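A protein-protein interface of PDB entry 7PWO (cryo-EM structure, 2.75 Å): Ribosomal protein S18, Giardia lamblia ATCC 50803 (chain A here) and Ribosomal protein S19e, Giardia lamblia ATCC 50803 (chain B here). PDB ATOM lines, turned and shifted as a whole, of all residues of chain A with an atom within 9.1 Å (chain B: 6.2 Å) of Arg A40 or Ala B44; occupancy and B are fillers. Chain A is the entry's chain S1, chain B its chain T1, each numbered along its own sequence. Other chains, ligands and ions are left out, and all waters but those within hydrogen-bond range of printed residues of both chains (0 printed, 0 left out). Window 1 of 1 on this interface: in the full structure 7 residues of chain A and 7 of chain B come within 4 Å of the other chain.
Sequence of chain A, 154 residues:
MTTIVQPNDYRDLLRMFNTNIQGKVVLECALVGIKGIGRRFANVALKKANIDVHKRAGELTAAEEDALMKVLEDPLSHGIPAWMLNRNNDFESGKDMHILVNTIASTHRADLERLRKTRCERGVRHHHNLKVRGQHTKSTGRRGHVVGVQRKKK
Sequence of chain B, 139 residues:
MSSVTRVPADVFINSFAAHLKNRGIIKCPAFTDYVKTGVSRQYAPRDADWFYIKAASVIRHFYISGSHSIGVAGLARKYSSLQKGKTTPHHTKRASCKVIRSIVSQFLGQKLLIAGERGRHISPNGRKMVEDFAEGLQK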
ATOM      1  N   GLU A  28      32.463  17.831 -12.730  1.00  0.00           N
ATOM      2  CA  GLU A  28      32.191  18.947 -11.830  1.00  0.00           C
ATOM      3  C   GLU A  28      32.571  18.615 -10.400  1.00  0.00           C
ATOM      4  O   GLU A  28      33.116  19.454  -9.681  1.00  0.00           O
ATOM      5  CB  GLU A  28      30.722  19.340 -11.882  1.00  0.00           C
ATOM      6  CG  GLU A  28      29.718  18.239 -11.594  1.00  0.00           C
ATOM      7  CD  GLU A  28      29.571  17.244 -12.721  1.00  0.00           C
ATOM      8  OE1 GLU A  28      28.825  16.261 -12.551  1.00  0.00           O
ATOM      9  OE2 GLU A  28      30.211  17.436 -13.773  1.00  0.00           O
ATOM     10  N   CYS A  29      32.271  17.397  -9.964  1.00  0.00           N
ATOM     11  CA  CYS A  29      32.623  17.004  -8.611  1.00  0.00           C
ATOM     12  C   CYS A  29      34.072  16.551  -8.538  1.00  0.00           C
ATOM     13  O   CYS A  29      34.784  16.898  -7.591  1.00  0.00           O
ATOM     14  CB  CYS A  29      31.671  15.915  -8.113  1.00  0.00           C
ATOM     15  SG  CYS A  29      29.914  16.251  -8.452  1.00  0.00           S
ATOM     16  N   LEU A  31      36.610  17.582 -10.013  1.00  0.00           N
ATOM     17  CA  LEU A  31      37.546  18.698  -9.963  1.00  0.00           C
ATOM     18  C   LEU A  31      37.712  19.235  -8.545  1.00  0.00           C
ATOM     19  O   LEU A  31      38.689  19.940  -8.271  1.00  0.00           O
ATOM     20  CB  LEU A  31      37.089  19.781 -10.952  1.00  0.00           C
ATOM     21  CG  LEU A  31      37.796  21.116 -11.193  1.00  0.00           C
ATOM     22  CD1 LEU A  31      37.316  21.699 -12.500  1.00  0.00           C
ATOM     23  CD2 LEU A  31      37.512  22.118 -10.120  1.00  0.00           C
ATOM     24  N   VAL A  32      36.796  18.896  -7.631  1.00  0.00           N
ATOM     25  CA  VAL A  32      36.977  19.210  -6.215  1.00  0.00           C
ATOM     26  C   VAL A  32      38.053  18.331  -5.592  1.00  0.00           C
ATOM     27  O   VAL A  32      38.442  18.546  -4.434  1.00  0.00           O
ATOM     28  CB  VAL A  32      35.595  19.089  -5.531  1.00  0.00           C
ATOM     29  CG1 VAL A  32      35.658  19.304  -4.025  1.00  0.00           C
ATOM     30  CG2 VAL A  32      34.586  20.032  -6.180  1.00  0.00           C
ATOM     31  N   GLY A  36      41.249  23.672  -2.245  1.00  0.00           N
ATOM     32  CA  GLY A  36      40.974  25.064  -2.523  1.00  0.00           C
ATOM     33  C   GLY A  36      39.814  25.312  -3.460  1.00  0.00           C
ATOM     34  O   GLY A  36      39.516  26.476  -3.753  1.00  0.00           O
ATOM     35  N   ILE A  37      39.155  24.264  -3.941  1.00  0.00           N
ATOM     36  CA  ILE A  37      38.077  24.383  -4.911  1.00  0.00           C
ATOM     37  C   ILE A  37      36.812  23.758  -4.330  1.00  0.00           C
ATOM     38  O   ILE A  37      36.874  22.804  -3.547  1.00  0.00           O
ATOM     39  CB  ILE A  37      38.448  23.703  -6.243  1.00  0.00           C
ATOM     40  CG1 ILE A  37      39.785  24.229  -6.777  1.00  0.00           C
ATOM     41  CG2 ILE A  37      37.385  23.972  -7.265  1.00  0.00           C
ATOM     42  CD1 ILE A  37      39.835  25.722  -6.974  1.00  0.00           C
ATOM     43  N   GLY A  38      35.653  24.306  -4.717  1.00  0.00           N
ATOM     44  CA  GLY A  38      34.371  23.727  -4.382  1.00  0.00           C
ATOM     45  C   GLY A  38      33.566  23.377  -5.628  1.00  0.00           C
ATOM     46  O   GLY A  38      33.926  23.736  -6.758  1.00  0.00           O
ATOM     47  N   ARG A  39      32.464  22.650  -5.402  1.00  0.00           N
ATOM     48  CA  ARG A  39      31.508  22.396  -6.478  1.00  0.00           C
ATOM     49  C   ARG A  39      31.010  23.694  -7.091  1.00  0.00           C
ATOM     50  O   ARG A  39      30.755  23.758  -8.301  1.00  0.00           O
ATOM     51  CB  ARG A  39      30.326  21.577  -5.957  1.00  0.00           C
ATOM     52  CG  ARG A  39      29.525  20.856  -7.038  1.00  0.00           C
ATOM     53  CD  ARG A  39      28.855  19.618  -6.480  1.00  0.00           C
ATOM     54  NE  ARG A  39      27.938  18.987  -7.427  1.00  0.00           N
ATOM     55  CZ  ARG A  39      27.088  18.017  -7.102  1.00  0.00           C
ATOM     56  NH1 ARG A  39      27.041  17.566  -5.856  1.00  0.00           N
ATOM     57  NH2 ARG A  39      26.288  17.493  -8.017  1.00  0.00           N
ATOM     58  N   ARG A  40      30.882  24.738  -6.275  1.00  0.00           N
ATOM     59  CA  ARG A  40      30.496  26.048  -6.785  1.00  0.00           C
ATOM     60  C   ARG A  40      31.505  26.557  -7.814  1.00  0.00           C
ATOM     61  O   ARG A  40      31.127  26.950  -8.925  1.00  0.00           O
ATOM     62  CB  ARG A  40      30.349  27.026  -5.617  1.00  0.00           C
ATOM     63  CG  ARG A  40      29.811  28.398  -5.987  1.00  0.00           C
ATOM     64  CD  ARG A  40      28.684  28.309  -7.003  1.00  0.00           C
ATOM     65  NE  ARG A  40      27.633  27.442  -6.503  1.00  0.00           N
ATOM     66  CZ  ARG A  40      26.503  27.860  -5.953  1.00  0.00           C
ATOM     67  NH1 ARG A  40      25.643  26.968  -5.516  1.00  0.00           N
ATOM     68  NH2 ARG A  40      26.235  29.155  -5.840  1.00  0.00           N
ATOM     69  N   PHE A  41      32.800  26.516  -7.476  1.00  0.00           N
ATOM     70  CA  PHE A  41      33.812  26.999  -8.408  1.00  0.00           C
ATOM     71  C   PHE A  41      33.919  26.104  -9.635  1.00  0.00           C
ATOM     72  O   PHE A  41      34.146  26.602 -10.740  1.00  0.00           O
ATOM     73  CB  PHE A  41      35.169  27.128  -7.715  1.00  0.00           C
ATOM     74  CG  PHE A  41      36.252  27.662  -8.607  1.00  0.00           C
ATOM     75  CD1 PHE A  41      36.298  29.009  -8.924  1.00  0.00           C
ATOM     76  CD2 PHE A  41      37.225  26.827  -9.121  1.00  0.00           C
ATOM     77  CE1 PHE A  41      37.273  29.510  -9.743  1.00  0.00           C
ATOM     78  CE2 PHE A  41      38.223  27.322  -9.939  1.00  0.00           C
ATOM     79  CZ  PHE A  41      38.246  28.666 -10.252  1.00  0.00           C
ATOM     80  N   ALA A  42      33.728  24.794  -9.474  1.00  0.00           N
ATOM     81  CA  ALA A  42      33.702  23.912 -10.635  1.00  0.00           C
ATOM     82  C   ALA A  42      32.597  24.311 -11.606  1.00  0.00           C
ATOM     83  O   ALA A  42      32.835  24.464 -12.813  1.00  0.00           O
ATOM     84  CB  ALA A  42      33.518  22.465 -10.188  1.00  0.00           C
ATOM     85  N   ASN A  43      31.374  24.484 -11.094  1.00  0.00           N
ATOM     86  CA  ASN A  43      30.265  24.818 -11.978  1.00  0.00           C
ATOM     87  C   ASN A  43      30.473  26.176 -12.636  1.00  0.00           C
ATOM     88  O   ASN A  43      30.201  26.338 -13.831  1.00  0.00           O
ATOM     89  CB  ASN A  43      28.935  24.782 -11.225  1.00  0.00           C
ATOM     90  CG  ASN A  43      27.737  24.919 -12.152  1.00  0.00           C
ATOM     91  OD1 ASN A  43      27.886  25.070 -13.365  1.00  0.00           O
ATOM     92  ND2 ASN A  43      26.547  24.870 -11.585  1.00  0.00           N
ATOM     93  N   VAL A  44      30.971  27.165 -11.889  1.00  0.00           N
ATOM     94  CA  VAL A  44      31.114  28.487 -12.497  1.00  0.00           C
ATOM     95  C   VAL A  44      32.414  28.606 -13.288  1.00  0.00           C
ATOM     96  O   VAL A  44      32.656  29.638 -13.920  1.00  0.00           O
ATOM     97  CB  VAL A  44      30.958  29.579 -11.413  1.00  0.00           C
ATOM     98  CG1 VAL A  44      31.977  29.424 -10.319  1.00  0.00           C
ATOM     99  CG2 VAL A  44      30.931  30.993 -11.995  1.00  0.00           C
ATOM    100  N   ALA A  45      33.259  27.571 -13.295  1.00  0.00           N
ATOM    101  CA  ALA A  45      34.435  27.582 -14.162  1.00  0.00           C
ATOM    102  C   ALA A  45      34.236  26.828 -15.473  1.00  0.00           C
ATOM    103  O   ALA A  45      34.650  27.330 -16.524  1.00  0.00           O
ATOM    104  CB  ALA A  45      35.643  26.993 -13.425  1.00  0.00           C
ATOM    105  N   LEU A  46      33.529  25.697 -15.473  1.00  0.00           N
ATOM    106  CA  LEU A  46      33.499  24.875 -16.688  1.00  0.00           C
ATOM    107  C   LEU A  46      32.657  25.496 -17.799  1.00  0.00           C
ATOM    108  O   LEU A  46      33.159  25.782 -18.890  1.00  0.00           O
ATOM    109  CB  LEU A  46      32.986  23.464 -16.381  1.00  0.00           C
ATOM    110  CG  LEU A  46      33.996  22.445 -15.847  1.00  0.00           C
ATOM    111  CD1 LEU A  46      35.049  22.204 -16.914  1.00  0.00           C
ATOM    112  CD2 LEU A  46      34.625  22.855 -14.548  1.00  0.00           C
ATOM    113  N   LYS A  47      31.361  25.690 -17.543  1.00  0.00           N
ATOM    114  CA  LYS A  47      30.490  26.253 -18.566  1.00  0.00           C
ATOM    115  C   LYS A  47      30.932  27.652 -18.995  1.00  0.00           C
ATOM    116  O   LYS A  47      30.750  28.019 -20.162  1.00  0.00           O
ATOM    117  CB  LYS A  47      29.037  26.183 -18.077  1.00  0.00           C
ATOM    118  CG  LYS A  47      28.728  26.991 -16.833  1.00  0.00           C
ATOM    119  CD  LYS A  47      28.294  28.384 -17.092  1.00  0.00           C
ATOM    120  CE  LYS A  47      27.933  29.012 -15.781  1.00  0.00           C
ATOM    121  NZ  LYS A  47      27.517  30.413 -15.945  1.00  0.00           N
ATOM    122  N   LYS A  48      31.555  28.428 -18.099  1.00  0.00           N
ATOM    123  CA  LYS A  48      32.238  29.642 -18.549  1.00  0.00           C
ATOM    124  C   LYS A  48      33.356  29.314 -19.526  1.00  0.00           C
ATOM    125  O   LYS A  48      33.524  30.001 -20.542  1.00  0.00           O
ATOM    126  CB  LYS A  48      32.784  30.446 -17.367  1.00  0.00           C
ATOM    127  CG  LYS A  48      31.737  30.950 -16.396  1.00  0.00           C
ATOM    128  CD  LYS A  48      30.761  31.901 -17.055  1.00  0.00           C
ATOM    129  CE  LYS A  48      31.430  33.202 -17.474  1.00  0.00           C
ATOM    130  NZ  LYS A  48      31.929  33.996 -16.317  1.00  0.00           N
ATOM    131  N   VAL A  53      29.358  20.202 -18.537  1.00  0.00           N
ATOM    132  CA  VAL A  53      29.809  19.965 -17.176  1.00  0.00           C
ATOM    133  C   VAL A  53      29.894  18.473 -16.874  1.00  0.00           C
ATOM    134  O   VAL A  53      30.864  18.015 -16.263  1.00  0.00           O
ATOM    135  CB  VAL A  53      28.891  20.691 -16.179  1.00  0.00           C
ATOM    136  CG1 VAL A  53      29.465  20.611 -14.804  1.00  0.00           C
ATOM    137  CG2 VAL A  53      28.666  22.144 -16.599  1.00  0.00           C
ATOM    138  N   ILE A  80      33.793  36.348 -13.245  1.00  0.00           N
ATOM    139  CA  ILE A  80      33.465  35.687 -11.976  1.00  0.00           C
ATOM    140  C   ILE A  80      33.430  36.739 -10.874  1.00  0.00           C
ATOM    141  O   ILE A  80      34.386  37.526 -10.739  1.00  0.00           O
ATOM    142  CB  ILE A  80      34.483  34.575 -11.666  1.00  0.00           C
ATOM    143  CG1 ILE A  80      34.796  33.789 -12.939  1.00  0.00           C
ATOM    144  CG2 ILE A  80      33.947  33.637 -10.589  1.00  0.00           C
ATOM    145  CD1 ILE A  80      35.898  32.769 -12.792  1.00  0.00           C
ATOM    146  N   PRO A  81      32.357  36.834 -10.095  1.00  0.00           N
ATOM    147  CA  PRO A  81      32.137  38.034  -9.276  1.00  0.00           C
ATOM    148  C   PRO A  81      33.033  38.066  -8.053  1.00  0.00           C
ATOM    149  O   PRO A  81      33.573  37.053  -7.614  1.00  0.00           O
ATOM    150  CB  PRO A  81      30.664  37.925  -8.870  1.00  0.00           C
ATOM    151  CG  PRO A  81      30.115  36.795  -9.664  1.00  0.00           C
ATOM    152  CD  PRO A  81      31.238  35.894  -9.985  1.00  0.00           C
ATOM    153  N   TRP A  83      32.239  38.426  -4.906  1.00  0.00           N
ATOM    154  CA  TRP A  83      31.711  37.677  -3.775  1.00  0.00           C
ATOM    155  C   TRP A  83      31.929  36.168  -3.892  1.00  0.00           C
ATOM    156  O   TRP A  83      31.789  35.460  -2.888  1.00  0.00           O
ATOM    157  CB  TRP A  83      30.233  38.019  -3.616  1.00  0.00           C
ATOM    158  CG  TRP A  83      29.433  37.866  -4.858  1.00  0.00           C
ATOM    159  CD1 TRP A  83      29.093  38.849  -5.738  1.00  0.00           C
ATOM    160  CD2 TRP A  83      28.822  36.663  -5.342  1.00  0.00           C
ATOM    161  NE1 TRP A  83      28.330  38.330  -6.752  1.00  0.00           N
ATOM    162  CE2 TRP A  83      28.150  36.990  -6.533  1.00  0.00           C
ATOM    163  CE3 TRP A  83      28.795  35.340  -4.893  1.00  0.00           C
ATOM    164  CZ2 TRP A  83      27.458  36.041  -7.280  1.00  0.00           C
ATOM    165  CZ3 TRP A  83      28.114  34.401  -5.634  1.00  0.00           C
ATOM    166  CH2 TRP A  83      27.456  34.752  -6.813  1.00  0.00           C
ATOM    167  N   MET A  84      32.263  35.652  -5.077  1.00  0.00           N
ATOM    168  CA  MET A  84      32.512  34.226  -5.246  1.00  0.00           C
ATOM    169  C   MET A  84      34.014  33.893  -5.329  1.00  0.00           C
ATOM    170  O   MET A  84      34.386  32.731  -5.520  1.00  0.00           O
ATOM    171  CB  MET A  84      31.729  33.718  -6.465  1.00  0.00           C
ATOM    172  CG  MET A  84      32.061  32.335  -6.993  1.00  0.00           C
ATOM    173  SD  MET A  84      30.587  31.448  -7.513  1.00  0.00           S
ATOM    174  CE  MET A  84      30.019  32.506  -8.829  1.00  0.00           C
ATOM    175  N   LEU A  85      34.888  34.863  -5.115  1.00  0.00           N
ATOM    176  CA  LEU A  85      36.304  34.545  -4.995  1.00  0.00           C
ATOM    177  C   LEU A  85      36.719  34.440  -3.535  1.00  0.00           C
ATOM    178  O   LEU A  85      35.995  34.828  -2.617  1.00  0.00           O
ATOM    179  CB  LEU A  85      37.193  35.546  -5.744  1.00  0.00           C
ATOM    180  CG  LEU A  85      37.333  35.420  -7.263  1.00  0.00           C
ATOM    181  CD1 LEU A  85      36.118  35.806  -8.023  1.00  0.00           C
ATOM    182  CD2 LEU A  85      38.515  36.256  -7.723  1.00  0.00           C
ATOM    183  N   ASN A  86      37.911  33.885  -3.334  1.00  0.00           N
ATOM    184  CA  ASN A  86      38.287  33.311  -2.049  1.00  0.00           C
ATOM    185  C   ASN A  86      39.023  34.296  -1.147  1.00  0.00           C
ATOM    186  O   ASN A  86      38.558  34.600  -0.045  1.00  0.00           O
ATOM    187  CB  ASN A  86      39.141  32.069  -2.300  1.00  0.00           C
ATOM    188  CG  ASN A  86      38.548  31.176  -3.362  1.00  0.00           C
ATOM    189  OD1 ASN A  86      38.865  31.307  -4.543  1.00  0.00           O
ATOM    190  ND2 ASN A  86      37.669  30.275  -2.954  1.00  0.00           N
ATOM    191  N   TYR B  34      25.846  32.484 -12.382  1.00  0.00           N
ATOM    192  CA  TYR B  34      26.248  32.676 -10.983  1.00  0.00           C
ATOM    193  C   TYR B  34      25.101  33.167 -10.097  1.00  0.00           C
ATOM    194  O   TYR B  34      25.259  34.085  -9.290  1.00  0.00           O
ATOM    195  CB  TYR B  34      27.476  33.592 -10.843  1.00  0.00           C
ATOM    196  CG  TYR B  34      27.478  34.911 -11.588  1.00  0.00           C
ATOM    197  CD1 TYR B  34      27.893  34.973 -12.914  1.00  0.00           C
ATOM    198  CD2 TYR B  34      27.215  36.109 -10.932  1.00  0.00           C
ATOM    199  CE1 TYR B  34      27.934  36.171 -13.598  1.00  0.00           C
ATOM    200  CE2 TYR B  34      27.256  37.324 -11.613  1.00  0.00           C
ATOM    201  CZ  TYR B  34      27.623  37.341 -12.949  1.00  0.00           C
ATOM    202  OH  TYR B  34      27.676  38.530 -13.637  1.00  0.00           O
ATOM    203  N   VAL B  35      23.939  32.525 -10.219  1.00  0.00           N
ATOM    204  CA  VAL B  35      22.836  32.768  -9.294  1.00  0.00           C
ATOM    205  C   VAL B  35      22.185  31.443  -8.911  1.00  0.00           C
ATOM    206  O   VAL B  35      21.985  30.563  -9.757  1.00  0.00           O
ATOM    207  CB  VAL B  35      21.788  33.748  -9.872  1.00  0.00           C
ATOM    208  CG1 VAL B  35      20.964  33.105 -10.976  1.00  0.00           C
ATOM    209  CG2 VAL B  35      20.902  34.292  -8.767  1.00  0.00           C
ATOM    210  N   LYS B  36      21.887  31.296  -7.619  1.00  0.00           N
ATOM    211  CA  LYS B  36      21.004  30.259  -7.109  1.00  0.00           C
ATOM    212  C   LYS B  36      19.611  30.839  -6.897  1.00  0.00           C
ATOM    213  O   LYS B  36      19.452  32.030  -6.625  1.00  0.00           O
ATOM    214  CB  LYS B  36      21.492  29.694  -5.776  1.00  0.00           C
ATOM    215  CG  LYS B  36      22.783  28.918  -5.808  1.00  0.00           C
ATOM    216  CD  LYS B  36      23.017  28.294  -4.443  1.00  0.00           C
ATOM    217  CE  LYS B  36      23.435  29.309  -3.414  1.00  0.00           C
ATOM    218  NZ  LYS B  36      23.769  28.679  -2.105  1.00  0.00           N
ATOM    219  N   THR B  37      18.602  29.975  -6.988  1.00  0.00           N
ATOM    220  CA  THR B  37      17.236  30.455  -6.815  1.00  0.00           C
ATOM    221  C   THR B  37      16.934  30.852  -5.379  1.00  0.00           C
ATOM    222  O   THR B  37      15.907  31.494  -5.143  1.00  0.00           O
ATOM    223  CB  THR B  37      16.231  29.408  -7.298  1.00  0.00           C
ATOM    224  OG1 THR B  37      16.329  28.227  -6.498  1.00  0.00           O
ATOM    225  CG2 THR B  37      16.521  29.047  -8.747  1.00  0.00           C
ATOM    226  N   ARG B  41      18.389  26.569  -1.470  1.00  0.00           N
ATOM    227  CA  ARG B  41      19.151  25.752  -2.406  1.00  0.00           C
ATOM    228  C   ARG B  41      20.645  26.024  -2.284  1.00  0.00           C
ATOM    229  O   ARG B  41      21.085  27.177  -2.301  1.00  0.00           O
ATOM    230  CB  ARG B  41      18.650  26.016  -3.826  1.00  0.00           C
ATOM    231  CG  ARG B  41      17.364  25.263  -4.163  1.00  0.00           C
ATOM    232  CD  ARG B  41      16.084  25.916  -3.648  1.00  0.00           C
ATOM    233  NE  ARG B  41      15.734  27.213  -4.210  1.00  0.00           N
ATOM    234  CZ  ARG B  41      14.803  28.002  -3.681  1.00  0.00           C
ATOM    235  NH1 ARG B  41      14.524  29.173  -4.227  1.00  0.00           N
ATOM    236  NH2 ARG B  41      14.155  27.621  -2.592  1.00  0.00           N
ATOM    237  N   GLN B  42      21.416  24.953  -2.128  1.00  0.00           N
ATOM    238  CA  GLN B  42      22.859  25.078  -1.988  1.00  0.00           C
ATOM    239  C   GLN B  42      23.575  25.170  -3.329  1.00  0.00           C
ATOM    240  O   GLN B  42      24.683  25.708  -3.382  1.00  0.00           O
ATOM    241  CB  GLN B  42      23.431  23.902  -1.187  1.00  0.00           C
ATOM    242  CG  GLN B  42      23.292  22.553  -1.859  1.00  0.00           C
ATOM    243  CD  GLN B  42      23.823  21.409  -1.006  1.00  0.00           C
ATOM    244  OE1 GLN B  42      24.353  21.622   0.083  1.00  0.00           O
ATOM    245  NE2 GLN B  42      23.674  20.188  -1.502  1.00  0.00           N
ATOM    246  N   TYR B  43      22.962  24.683  -4.408  1.00  0.00           N
ATOM    247  CA  TYR B  43      23.526  24.776  -5.746  1.00  0.00           C
ATOM    248  C   TYR B  43      22.612  25.580  -6.653  1.00  0.00           C
ATOM    249  O   TYR B  43      21.393  25.620  -6.464  1.00  0.00           O
ATOM    250  CB  TYR B  43      23.754  23.396  -6.368  1.00  0.00           C
ATOM    251  CG  TYR B  43      24.506  22.450  -5.474  1.00  0.00           C
ATOM    252  CD1 TYR B  43      25.634  22.870  -4.778  1.00  0.00           C
ATOM    253  CD2 TYR B  43      24.091  21.130  -5.321  1.00  0.00           C
ATOM    254  CE1 TYR B  43      26.319  22.006  -3.957  1.00  0.00           C
ATOM    255  CE2 TYR B  43      24.770  20.265  -4.505  1.00  0.00           C
ATOM    256  CZ  TYR B  43      25.886  20.706  -3.825  1.00  0.00           C
ATOM    257  OH  TYR B  43      26.571  19.841  -3.008  1.00  0.00           O
ATOM    258  N   ALA B  44      23.212  26.220  -7.648  1.00  0.00           N
ATOM    259  CA  ALA B  44      22.428  26.754  -8.740  1.00  0.00           C
ATOM    260  C   ALA B  44      21.799  25.593  -9.501  1.00  0.00           C
ATOM    261  O   ALA B  44      22.330  24.478  -9.493  1.00  0.00           O
ATOM    262  CB  ALA B  44      23.294  27.595  -9.676  1.00  0.00           C
ATOM    263  N   PRO B  45      20.656  25.817 -10.145  1.00  0.00           N
ATOM    264  CA  PRO B  45      20.045  24.758 -10.952  1.00  0.00           C
ATOM    265  C   PRO B  45      20.993  24.279 -12.037  1.00  0.00           C
ATOM    266  O   PRO B  45      22.081  24.821 -12.251  1.00  0.00           O
ATOM    267  CB  PRO B  45      18.798  25.425 -11.542  1.00  0.00           C
ATOM    268  CG  PRO B  45      18.971  26.866 -11.300  1.00  0.00           C
ATOM    269  CD  PRO B  45      19.820  27.025 -10.102  1.00  0.00           C
ATOM    270  N   ARG B  46      20.576  23.219 -12.717  1.00  0.00           N
ATOM    271  CA  ARG B  46      21.465  22.523 -13.633  1.00  0.00           C
ATOM    272  C   ARG B  46      20.977  22.564 -15.071  1.00  0.00           C
ATOM    273  O   ARG B  46      21.760  22.879 -15.975  1.00  0.00           O
ATOM    274  CB  ARG B  46      21.665  21.071 -13.162  1.00  0.00           C
ATOM    275  CG  ARG B  46      20.423  20.210 -13.169  1.00  0.00           C
ATOM    276  CD  ARG B  46      20.812  18.761 -13.152  1.00  0.00           C
ATOM    277  NE  ARG B  46      21.206  18.329 -14.486  1.00  0.00           N
ATOM    278  CZ  ARG B  46      21.048  17.100 -14.950  1.00  0.00           C
ATOM    279  NH1 ARG B  46      21.440  16.806 -16.182  1.00  0.00           N
ATOM    280  NH2 ARG B  46      20.474  16.180 -14.192  1.00  0.00           N
ATOM    281  N   TRP B  50      16.469  26.606 -17.207  1.00  0.00           N
ATOM    282  CA  TRP B  50      15.706  26.842 -15.991  1.00  0.00           C
ATOM    283  C   TRP B  50      15.139  28.249 -15.909  1.00  0.00           C
ATOM    284  O   TRP B  50      14.170  28.458 -15.183  1.00  0.00           O
ATOM    285  CB  TRP B  50      16.570  26.617 -14.753  1.00  0.00           C
ATOM    286  CG  TRP B  50      17.718  27.545 -14.708  1.00  0.00           C
ATOM    287  CD1 TRP B  50      18.786  27.567 -15.541  1.00  0.00           C
ATOM    288  CD2 TRP B  50      17.851  28.685 -13.854  1.00  0.00           C
ATOM    289  NE1 TRP B  50      19.620  28.607 -15.211  1.00  0.00           N
ATOM    290  CE2 TRP B  50      19.065  29.307 -14.177  1.00  0.00           C
ATOM    291  CE3 TRP B  50      17.078  29.212 -12.816  1.00  0.00           C
ATOM    292  CZ2 TRP B  50      19.520  30.435 -13.510  1.00  0.00           C
ATOM    293  CZ3 TRP B  50      17.537  30.327 -12.155  1.00  0.00           C
ATOM    294  CH2 TRP B  50      18.738  30.932 -12.504  1.00  0.00           C
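Printed residues of chain B within 4 Å of Arg A39: Tyr B43 (3.7 Å). Arg A40 touches just these residues of chain B: Lys B36 (3.1 Å), Gln B42 (2.7 Å), Tyr B43 (3.1 Å) and Ala B44 (3.3 Å). Lys A47 touches none of the printed residues of chain B. Of the printed residues of chain B, Trp A83 touches Tyr B34 (3.4 Å). Printed residues of chain A within 4 Å of Lys B36: Arg A40. Of the printed residues of chain A, Tyr B43 touches Arg A39 and Arg A40. Of chain A, only Arg A40 (3.3 Å) comes within 4 Å of Ala B44. No residue of chain A comes within 4 Å of Pro B45. The nearest printed residue of chain B that does not touch Arg A40 is Val B35 (5.6 Å). The nearest residue of chain A that does not touch Ala B44 is Asn A43 (4.7 Å).
Among the printed residues, pairs that only touch across the chains: Arg A40 with Tyr B43, Arg A40 with Lys B36, Pro A81 with Tyr B34, Trp A83 with Tyr B34, Met A84 with Tyr B34 and Arg A39 with Tyr B43.
The side-chain sulfur (SG) of Cys A29 lies within hydrogen-bond range of the guanidinium group (NE) of Arg A39, 3.5 Å away. The side-chain hydroxyl of Tyr B43 lies close to the side-chain amide nitrogen of Gln B42 (3.3 Å). The side-chain amino group (NZ) of Lys B36 sits close to the backbone carbonyl oxygen (O) of Gln B42 (3.4 Å). The backbone carbonyl oxygen (O) of Arg B41 sits at hydrogen-bond distance from the side-chain amino group (NZ) of Lys B36, at 3.1 Å.
O of Gln B42 is in hydrogen-bond range of NH1 of Arg A40. The guanidinium group (NH1) of Arg A40 lies close to the backbone NH (N) of Ala B44 (3.3 Å).
Printed residues of chain B that touch a printed residue of chain A: Tyr B34, Lys B36, Gln B42, Tyr B43 and Ala B44. Hydrophobic or aromatic side chains of chain B that line the printed part of chain A: Tyr B34 and Tyr B43. Printed residues of chain A that touch a printed residue of chain B: Arg A39, Arg A40, Pro A81, Trp A83 and Met A84. Hydrophobic or aromatic side chains of chain A within 4 Å of the printed part of chain B: Pro A81, Trp A83 and Met A84. Among the printed residues, no Asp or Glu carboxylate lies within 4 Å of a Lys or Arg side-chain nitrogen of the other chain.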
